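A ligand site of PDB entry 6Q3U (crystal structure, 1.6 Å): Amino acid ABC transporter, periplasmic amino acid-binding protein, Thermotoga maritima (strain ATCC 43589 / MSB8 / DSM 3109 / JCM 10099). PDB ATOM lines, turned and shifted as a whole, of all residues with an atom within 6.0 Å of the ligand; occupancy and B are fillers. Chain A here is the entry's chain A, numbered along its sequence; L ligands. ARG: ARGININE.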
ATOM      1  N   LEU A  15      33.198   6.926   3.464  1.00  0.00           N
ATOM      2  CA  LEU A  15      32.138   7.735   4.151  1.00  0.00           C
ATOM      3  C   LEU A  15      32.749   8.299   5.424  1.00  0.00           C
ATOM      4  O   LEU A  15      33.904   8.001   5.757  1.00  0.00           O
ATOM      5  CB  LEU A  15      30.933   6.879   4.446  1.00  0.00           C
ATOM      6  CG  LEU A  15      31.192   5.546   5.196  1.00  0.00           C
ATOM      7  CD1 LEU A  15      31.528   5.691   6.619  1.00  0.00           C
ATOM      8  CD2 LEU A  15      29.921   4.656   5.047  1.00  0.00           C
ATOM      9  N   SER A  16      31.976   9.179   6.059  1.00  0.00           N
ATOM     10  CA  SER A  16      32.265   9.701   7.376  1.00  0.00           C
ATOM     11  C   SER A  16      31.176   9.255   8.296  1.00  0.00           C
ATOM     12  O   SER A  16      30.012   9.713   8.195  1.00  0.00           O
ATOM     13  CB  SER A  16      32.309  11.262   7.312  1.00  0.00           C
ATOM     14  OG  SER A  16      32.445  11.800   8.625  1.00  0.00           O
ATOM     15  N   ALA A  17      31.545   8.388   9.228  1.00  0.00           N
ATOM     16  CA  ALA A  17      30.527   7.691  10.033  1.00  0.00           C
ATOM     17  C   ALA A  17      30.094   8.510  11.259  1.00  0.00           C
ATOM     18  O   ALA A  17      30.215   8.025  12.431  1.00  0.00           O
ATOM     19  CB  ALA A  17      30.997   6.333  10.426  1.00  0.00           C
ATOM     20  N   ASP A  18      29.589   9.697  11.006  1.00  0.00           N
ATOM     21  CA  ASP A  18      29.117  10.605  12.081  1.00  0.00           C
ATOM     22  C   ASP A  18      27.803  11.217  11.662  1.00  0.00           C
ATOM     23  O   ASP A  18      27.531  12.365  11.947  1.00  0.00           O
ATOM     24  CB  ASP A  18      30.152  11.682  12.381  1.00  0.00           C
ATOM     25  CG  ASP A  18      30.489  12.530  11.148  1.00  0.00           C
ATOM     26  OD1 ASP A  18      30.128  12.232   9.983  1.00  0.00           O
ATOM     27  OD2 ASP A  18      31.195  13.537  11.317  1.00  0.00           O
ATOM     28  N   PHE A  19      26.965  10.412  10.978  1.00  0.00           N
ATOM     29  CA  PHE A  19      25.841  10.914  10.252  1.00  0.00           C
ATOM     30  C   PHE A  19      24.638   9.943  10.262  1.00  0.00           C
ATOM     31  O   PHE A  19      24.172   9.476   9.187  1.00  0.00           O
ATOM     32  CB  PHE A  19      26.277  11.227   8.812  1.00  0.00           C
ATOM     33  CG  PHE A  19      25.452  12.230   8.089  1.00  0.00           C
ATOM     34  CD1 PHE A  19      25.453  13.567   8.481  1.00  0.00           C
ATOM     35  CD2 PHE A  19      24.680  11.923   6.962  1.00  0.00           C
ATOM     36  CE1 PHE A  19      24.740  14.572   7.751  1.00  0.00           C
ATOM     37  CE2 PHE A  19      23.924  12.892   6.293  1.00  0.00           C
ATOM     38  CZ  PHE A  19      23.981  14.247   6.661  1.00  0.00           C
ATOM     39  N   GLU A  23      25.121   6.727   8.284  1.00  0.00           N
ATOM     40  CA  GLU A  23      26.248   5.986   8.720  1.00  0.00           C
ATOM     41  C   GLU A  23      26.671   6.474  10.081  1.00  0.00           C
ATOM     42  O   GLU A  23      26.749   7.721  10.331  1.00  0.00           O
ATOM     43  CB  GLU A  23      27.469   6.107   7.771  1.00  0.00           C
ATOM     44  CG  GLU A  23      27.781   7.580   7.328  1.00  0.00           C
ATOM     45  CD  GLU A  23      26.977   8.023   6.089  1.00  0.00           C
ATOM     46  OE1 GLU A  23      26.706   7.063   5.256  1.00  0.00           O
ATOM     47  OE2 GLU A  23      26.670   9.223   5.912  1.00  0.00           O
ATOM     48  N   PHE A  57      34.731  13.879   6.304  1.00  0.00           N
ATOM     49  CA  PHE A  57      33.807  14.124   5.223  1.00  0.00           C
ATOM     50  C   PHE A  57      34.458  14.947   4.135  1.00  0.00           C
ATOM     51  O   PHE A  57      34.327  14.639   2.958  1.00  0.00           O
ATOM     52  CB  PHE A  57      32.542  14.811   5.704  1.00  0.00           C
ATOM     53  CG  PHE A  57      31.614  15.151   4.619  1.00  0.00           C
ATOM     54  CD1 PHE A  57      30.753  14.141   4.084  1.00  0.00           C
ATOM     55  CD2 PHE A  57      31.528  16.420   4.089  1.00  0.00           C
ATOM     56  CE1 PHE A  57      29.931  14.389   3.035  1.00  0.00           C
ATOM     57  CE2 PHE A  57      30.670  16.667   2.999  1.00  0.00           C
ATOM     58  CZ  PHE A  57      29.834  15.668   2.495  1.00  0.00           C
ATOM     59  N   LEU A  60      36.605  13.086   1.525  1.00  0.00           N
ATOM     60  CA  LEU A  60      36.068  12.045   0.715  1.00  0.00           C
ATOM     61  C   LEU A  60      36.317  12.237  -0.796  1.00  0.00           C
ATOM     62  O   LEU A  60      36.744  11.326  -1.524  1.00  0.00           O
ATOM     63  CB  LEU A  60      34.542  11.909   0.957  1.00  0.00           C
ATOM     64  CG  LEU A  60      34.165  11.328   2.307  1.00  0.00           C
ATOM     65  CD1 LEU A  60      32.690  11.631   2.534  1.00  0.00           C
ATOM     66  CD2 LEU A  60      34.446   9.768   2.320  1.00  0.00           C
ATOM     67  N   SER A  74      27.769   8.525   1.470  1.00  0.00           N
ATOM     68  CA  SER A  74      28.029   9.181   2.718  1.00  0.00           C
ATOM     69  C   SER A  74      27.053  10.334   2.949  1.00  0.00           C
ATOM     70  O   SER A  74      27.447  11.407   3.457  1.00  0.00           O
ATOM     71  CB  SER A  74      29.463   9.704   2.817  1.00  0.00           C
ATOM     72  OG  SER A  74      29.806  10.029   4.146  1.00  0.00           O
ATOM     73  N   GLY A  75      25.776  10.135   2.559  1.00  0.00           N
ATOM     74  CA  GLY A  75      24.795  11.174   2.711  1.00  0.00           C
ATOM     75  C   GLY A  75      25.168  12.422   1.967  1.00  0.00           C
ATOM     76  O   GLY A  75      24.868  13.564   2.435  1.00  0.00           O
ATOM     77  N   MET A  76      25.864  12.271   0.832  1.00  0.00           N
ATOM     78  CA  MET A  76      26.363  13.398   0.079  1.00  0.00           C
ATOM     79  C   MET A  76      25.412  14.010  -0.912  1.00  0.00           C
ATOM     80  O   MET A  76      24.806  13.343  -1.782  1.00  0.00           O
ATOM     81  CB  MET A  76      27.658  12.962  -0.672  1.00  0.00           C
ATOM     82  CG  MET A  76      28.259  14.143  -1.426  1.00  0.00           C
ATOM     83  SD  MET A  76      29.912  13.780  -2.109  1.00  0.00           S
ATOM     84  CE  MET A  76      30.964  14.026  -0.708  1.00  0.00           C
ATOM     85  N   THR A  77      25.148  15.323  -0.727  1.00  0.00           N
ATOM     86  CA  THR A  77      24.301  16.093  -1.600  1.00  0.00           C
ATOM     87  C   THR A  77      24.966  16.256  -2.965  1.00  0.00           C
ATOM     88  O   THR A  77      26.113  16.641  -3.097  1.00  0.00           O
ATOM     89  CB  THR A  77      24.047  17.497  -0.982  1.00  0.00           C
ATOM     90  OG1 THR A  77      23.424  17.282   0.291  1.00  0.00           O
ATOM     91  CG2 THR A  77      23.201  18.305  -1.871  1.00  0.00           C
ATOM     92  N   ILE A  78      24.115  16.099  -3.929  1.00  0.00           N
ATOM     93  CA  ILE A  78      24.469  16.400  -5.324  1.00  0.00           C
ATOM     94  C   ILE A  78      24.400  17.911  -5.466  1.00  0.00           C
ATOM     95  O   ILE A  78      23.313  18.468  -5.337  1.00  0.00           O
ATOM     96  CB  ILE A  78      23.446  15.745  -6.247  1.00  0.00           C
ATOM     97  CG1 ILE A  78      23.379  14.214  -6.078  1.00  0.00           C
ATOM     98  CG2 ILE A  78      23.825  16.083  -7.731  1.00  0.00           C
ATOM     99  CD1 ILE A  78      22.194  13.588  -6.636  1.00  0.00           C
ATOM    100  N   ARG A  82      30.025  20.263  -6.916  1.00  0.00           N
ATOM    101  CA  ARG A  82      30.707  18.966  -6.855  1.00  0.00           C
ATOM    102  C   ARG A  82      30.657  18.252  -8.228  1.00  0.00           C
ATOM    103  O   ARG A  82      31.586  17.457  -8.498  1.00  0.00           O
ATOM    104  CB  ARG A  82      30.133  18.049  -5.752  1.00  0.00           C
ATOM    105  CG  ARG A  82      30.419  18.554  -4.342  1.00  0.00           C
ATOM    106  CD  ARG A  82      29.421  17.940  -3.321  1.00  0.00           C
ATOM    107  NE  ARG A  82      29.713  18.484  -2.028  1.00  0.00           N
ATOM    108  CZ  ARG A  82      28.968  18.269  -0.935  1.00  0.00           C
ATOM    109  NH1 ARG A  82      27.897  17.561  -1.022  1.00  0.00           N
ATOM    110  NH2 ARG A  82      29.356  18.734   0.226  1.00  0.00           N
ATOM    111  N   GLN A  97      18.703  21.686   4.891  1.00  0.00           N
ATOM    112  CA  GLN A  97      19.348  22.129   6.152  1.00  0.00           C
ATOM    113  C   GLN A  97      18.325  22.576   7.196  1.00  0.00           C
ATOM    114  O   GLN A  97      17.297  23.163   6.828  1.00  0.00           O
ATOM    115  CB  GLN A  97      20.311  23.254   5.904  1.00  0.00           C
ATOM    116  CG  GLN A  97      21.450  22.971   4.934  1.00  0.00           C
ATOM    117  CD  GLN A  97      22.253  21.786   5.352  1.00  0.00           C
ATOM    118  OE1 GLN A  97      22.838  21.720   6.400  1.00  0.00           O
ATOM    119  NE2 GLN A  97      22.236  20.772   4.503  1.00  0.00           N
ATOM    120  N   GLN A 123      29.850  21.038  10.101  1.00  0.00           N
ATOM    121  CA  GLN A 123      30.920  20.134   9.667  1.00  0.00           C
ATOM    122  C   GLN A 123      31.590  20.664   8.387  1.00  0.00           C
ATOM    123  O   GLN A 123      30.932  21.135   7.412  1.00  0.00           O
ATOM    124  CB  GLN A 123      30.348  18.740   9.340  1.00  0.00           C
ATOM    125  CG  GLN A 123      31.371  17.797   8.610  1.00  0.00           C
ATOM    126  CD  GLN A 123      30.821  16.417   8.565  1.00  0.00           C
ATOM    127  OE1 GLN A 123      29.932  16.145   7.755  1.00  0.00           O
ATOM    128  NE2 GLN A 123      31.278  15.542   9.423  1.00  0.00           N
ATOM    129  N   GLY A 125      33.105  21.541   5.011  1.00  0.00           N
ATOM    130  CA  GLY A 125      32.917  21.140   3.664  1.00  0.00           C
ATOM    131  C   GLY A 125      31.522  20.599   3.302  1.00  0.00           C
ATOM    132  O   GLY A 125      31.251  20.258   2.125  1.00  0.00           O
ATOM    133  N   THR A 126      30.597  20.666   4.287  1.00  0.00           N
ATOM    134  CA  THR A 126      29.201  20.314   3.986  1.00  0.00           C
ATOM    135  C   THR A 126      28.422  21.465   3.356  1.00  0.00           C
ATOM    136  O   THR A 126      28.838  22.637   3.366  1.00  0.00           O
ATOM    137  CB  THR A 126      28.456  19.898   5.264  1.00  0.00           C
ATOM    138  OG1 THR A 126      28.466  21.040   6.168  1.00  0.00           O
ATOM    139  CG2 THR A 126      29.078  18.672   5.896  1.00  0.00           C
ATOM    140  N   THR A 127      27.252  21.124   2.809  1.00  0.00           N
ATOM    141  CA  THR A 127      26.355  22.086   2.248  1.00  0.00           C
ATOM    142  C   THR A 127      25.938  23.084   3.339  1.00  0.00           C
ATOM    143  O   THR A 127      25.752  24.309   3.034  1.00  0.00           O
ATOM    144  CB  THR A 127      25.151  21.432   1.592  1.00  0.00           C
ATOM    145  OG1 THR A 127      24.582  20.427   2.421  1.00  0.00           O
ATOM    146  CG2 THR A 127      25.544  20.817   0.270  1.00  0.00           C
ATOM    147  N   GLY A 128      25.848  22.605   4.589  1.00  0.00           N
ATOM    148  CA  GLY A 128      25.604  23.520   5.740  1.00  0.00           C
ATOM    149  C   GLY A 128      26.701  24.571   5.902  1.00  0.00           C
ATOM    150  O   GLY A 128      26.388  25.802   6.003  1.00  0.00           O
ATOM    151  N   PHE A 146      30.916  15.742  13.114  1.00  0.00           N
ATOM    152  CA  PHE A 146      29.717  16.262  13.685  1.00  0.00           C
ATOM    153  C   PHE A 146      29.616  16.125  15.196  1.00  0.00           C
ATOM    154  O   PHE A 146      28.991  16.959  15.863  1.00  0.00           O
ATOM    155  CB  PHE A 146      28.448  15.644  13.021  1.00  0.00           C
ATOM    156  CG  PHE A 146      27.924  16.456  11.878  1.00  0.00           C
ATOM    157  CD1 PHE A 146      27.472  17.782  12.016  1.00  0.00           C
ATOM    158  CD2 PHE A 146      27.833  15.843  10.600  1.00  0.00           C
ATOM    159  CE1 PHE A 146      27.046  18.537  10.945  1.00  0.00           C
ATOM    160  CE2 PHE A 146      27.339  16.552   9.559  1.00  0.00           C
ATOM    161  CZ  PHE A 146      26.999  17.892   9.673  1.00  0.00           C
ATOM    162  N   ASP A 164      21.890  18.840   7.930  1.00  0.00           N
ATOM    163  CA  ASP A 164      20.741  18.206   7.274  1.00  0.00           C
ATOM    164  C   ASP A 164      19.683  17.696   8.243  1.00  0.00           C
ATOM    165  O   ASP A 164      20.002  17.081   9.281  1.00  0.00           O
ATOM    166  CB  ASP A 164      21.203  16.973   6.455  1.00  0.00           C
ATOM    167  CG  ASP A 164      22.291  17.266   5.412  1.00  0.00           C
ATOM    168  OD1 ASP A 164      23.210  18.080   5.634  1.00  0.00           O
ATOM    169  OD2 ASP A 164      22.265  16.555   4.386  1.00  0.00           O
ATOM    170  N   GLU A 188      17.703  19.514  -1.025  1.00  0.00           N
ATOM    171  CA  GLU A 188      18.876  18.731  -1.408  1.00  0.00           C
ATOM    172  C   GLU A 188      18.508  17.270  -1.673  1.00  0.00           C
ATOM    173  O   GLU A 188      17.511  16.766  -1.120  1.00  0.00           O
ATOM    174  CB  GLU A 188      19.946  18.823  -0.330  1.00  0.00           C
ATOM    175  CG  GLU A 188      20.435  20.245  -0.096  1.00  0.00           C
ATOM    176  CD  GLU A 188      21.408  20.409   1.081  1.00  0.00           C
ATOM    177  OE1 GLU A 188      22.319  19.603   1.303  1.00  0.00           O
ATOM    178  OE2 GLU A 188      21.317  21.479   1.791  1.00  0.00           O
ATOM    179  N   TYR A 190      20.546  13.390  -2.033  1.00  0.00           N
ATOM    180  CA  TYR A 190      21.763  12.600  -1.908  1.00  0.00           C
ATOM    181  C   TYR A 190      22.004  11.722  -3.122  1.00  0.00           C
ATOM    182  O   TYR A 190      21.080  11.159  -3.692  1.00  0.00           O
ATOM    183  CB  TYR A 190      21.728  11.705  -0.658  1.00  0.00           C
ATOM    184  CG  TYR A 190      21.576  12.407   0.662  1.00  0.00           C
ATOM    185  CD1 TYR A 190      21.713  13.787   0.801  1.00  0.00           C
ATOM    186  CD2 TYR A 190      21.346  11.636   1.833  1.00  0.00           C
ATOM    187  CE1 TYR A 190      21.513  14.396   2.018  1.00  0.00           C
ATOM    188  CE2 TYR A 190      21.254  12.247   3.105  1.00  0.00           C
ATOM    189  CZ  TYR A 190      21.291  13.615   3.154  1.00  0.00           C
ATOM    190  OH  TYR A 190      21.112  14.255   4.395  1.00  0.00           O
HETATM  191  N   ARG L   1      24.433  16.310   2.705  1.00  0.00           N
HETATM  192  CA  ARG L   1      25.466  17.223   3.319  1.00  0.00           C
HETATM  193  C   ARG L   1      26.584  17.421   2.290  1.00  0.00           C
HETATM  194  O   ARG L   1      27.466  18.269   2.408  1.00  0.00           O
HETATM  195  CB  ARG L   1      26.050  16.675   4.580  1.00  0.00           C
HETATM  196  CG  ARG L   1      26.633  15.287   4.477  1.00  0.00           C
HETATM  197  CD  ARG L   1      27.565  14.901   5.605  1.00  0.00           C
HETATM  198  NE  ARG L   1      27.768  13.433   5.638  1.00  0.00           N
HETATM  199  CZ  ARG L   1      28.452  12.767   6.532  1.00  0.00           C
HETATM  200  NH1 ARG L   1      28.517  11.467   6.463  1.00  0.00           N
HETATM  201  NH2 ARG L   1      29.075  13.448   7.519  1.00  0.00           N
HETATM  202  OXT ARG L   1      26.582  16.690   1.261  1.00  0.00           O
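The side-chain carboxylate (OD2) of Asp 164 lies within hydrogen-bond range of the side-chain hydroxyl (OH) of Tyr 190 (2.6 Å). OD1 of Asp 164 is in hydrogen-bond range of NE2 of Gln 97. O of Thr 77 is in hydrogen-bond range of NH1 of Arg 82, 2.9 Å away. OG1 of Thr 77 is in hydrogen-bond range of OE1 of Glu 188, at 2.8 Å. The side-chain carboxylate of Asp 18 sits at hydrogen-bond distance from the side-chain amide nitrogen of Gln 123 (2.8 Å). NE2 of Gln 97 is in hydrogen-bond range of OG1 of Thr 127, 3.2 Å away. N of Phe 146 sits at hydrogen-bond distance from OD2 of Asp 18 (2.9 Å). OG1 of Thr 126 lies close to N of Gly 128.
Residues that only touch the ligand: Thr 126 (3.1 Å), Phe 19 (3.3 Å), Phe 57 (3.4 Å), Met 76 (3.5 Å) and Tyr 190 (3.6 Å). Hydrophobic or aromatic side chains that line the ligand: Phe 19, Phe 57 and Tyr 190.
OD2 of Asp 164 lies within salt-bridge range of N of the ligand, 2.8 Å away. An oxygen (OXT) of the ligand is in salt-bridge range of the guanidinium group (NH1) of Arg 82 (2.8 Å). The backbone NH (N) of Thr 77 lies within hydrogen-bond range of an oxygen (OXT) of the ligand. OG1 of Thr 77 is in hydrogen-bond range of N of the ligand, at 2.8 Å. The backbone carbonyl oxygen of Gly 75 lies within hydrogen-bond range of a nitrogen (N) of the ligand (2.8 Å). OE1 of Gln 123 lies within hydrogen-bond range of NH2 of the ligand, 2.8 Å away. A nitrogen (NH1) of the ligand sits at hydrogen-bond distance from the backbone carbonyl oxygen of Ser 16 (2.9 Å). N of Thr 127 lies within hydrogen-bond range of O of the ligand, 2.9 Å away. The side-chain carboxylate of Asp 18 is in salt-bridge range of a nitrogen (NH2) of the ligand (2.9 Å). The side-chain carboxylate of Glu 23 is in salt-bridge range of a nitrogen (NH1) of the ligand. NE of the ligand is in hydrogen-bond range of O of Ser 74. The side-chain hydroxyl of Ser 74 sits at hydrogen-bond distance from a nitrogen (NH1) of the ligand.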
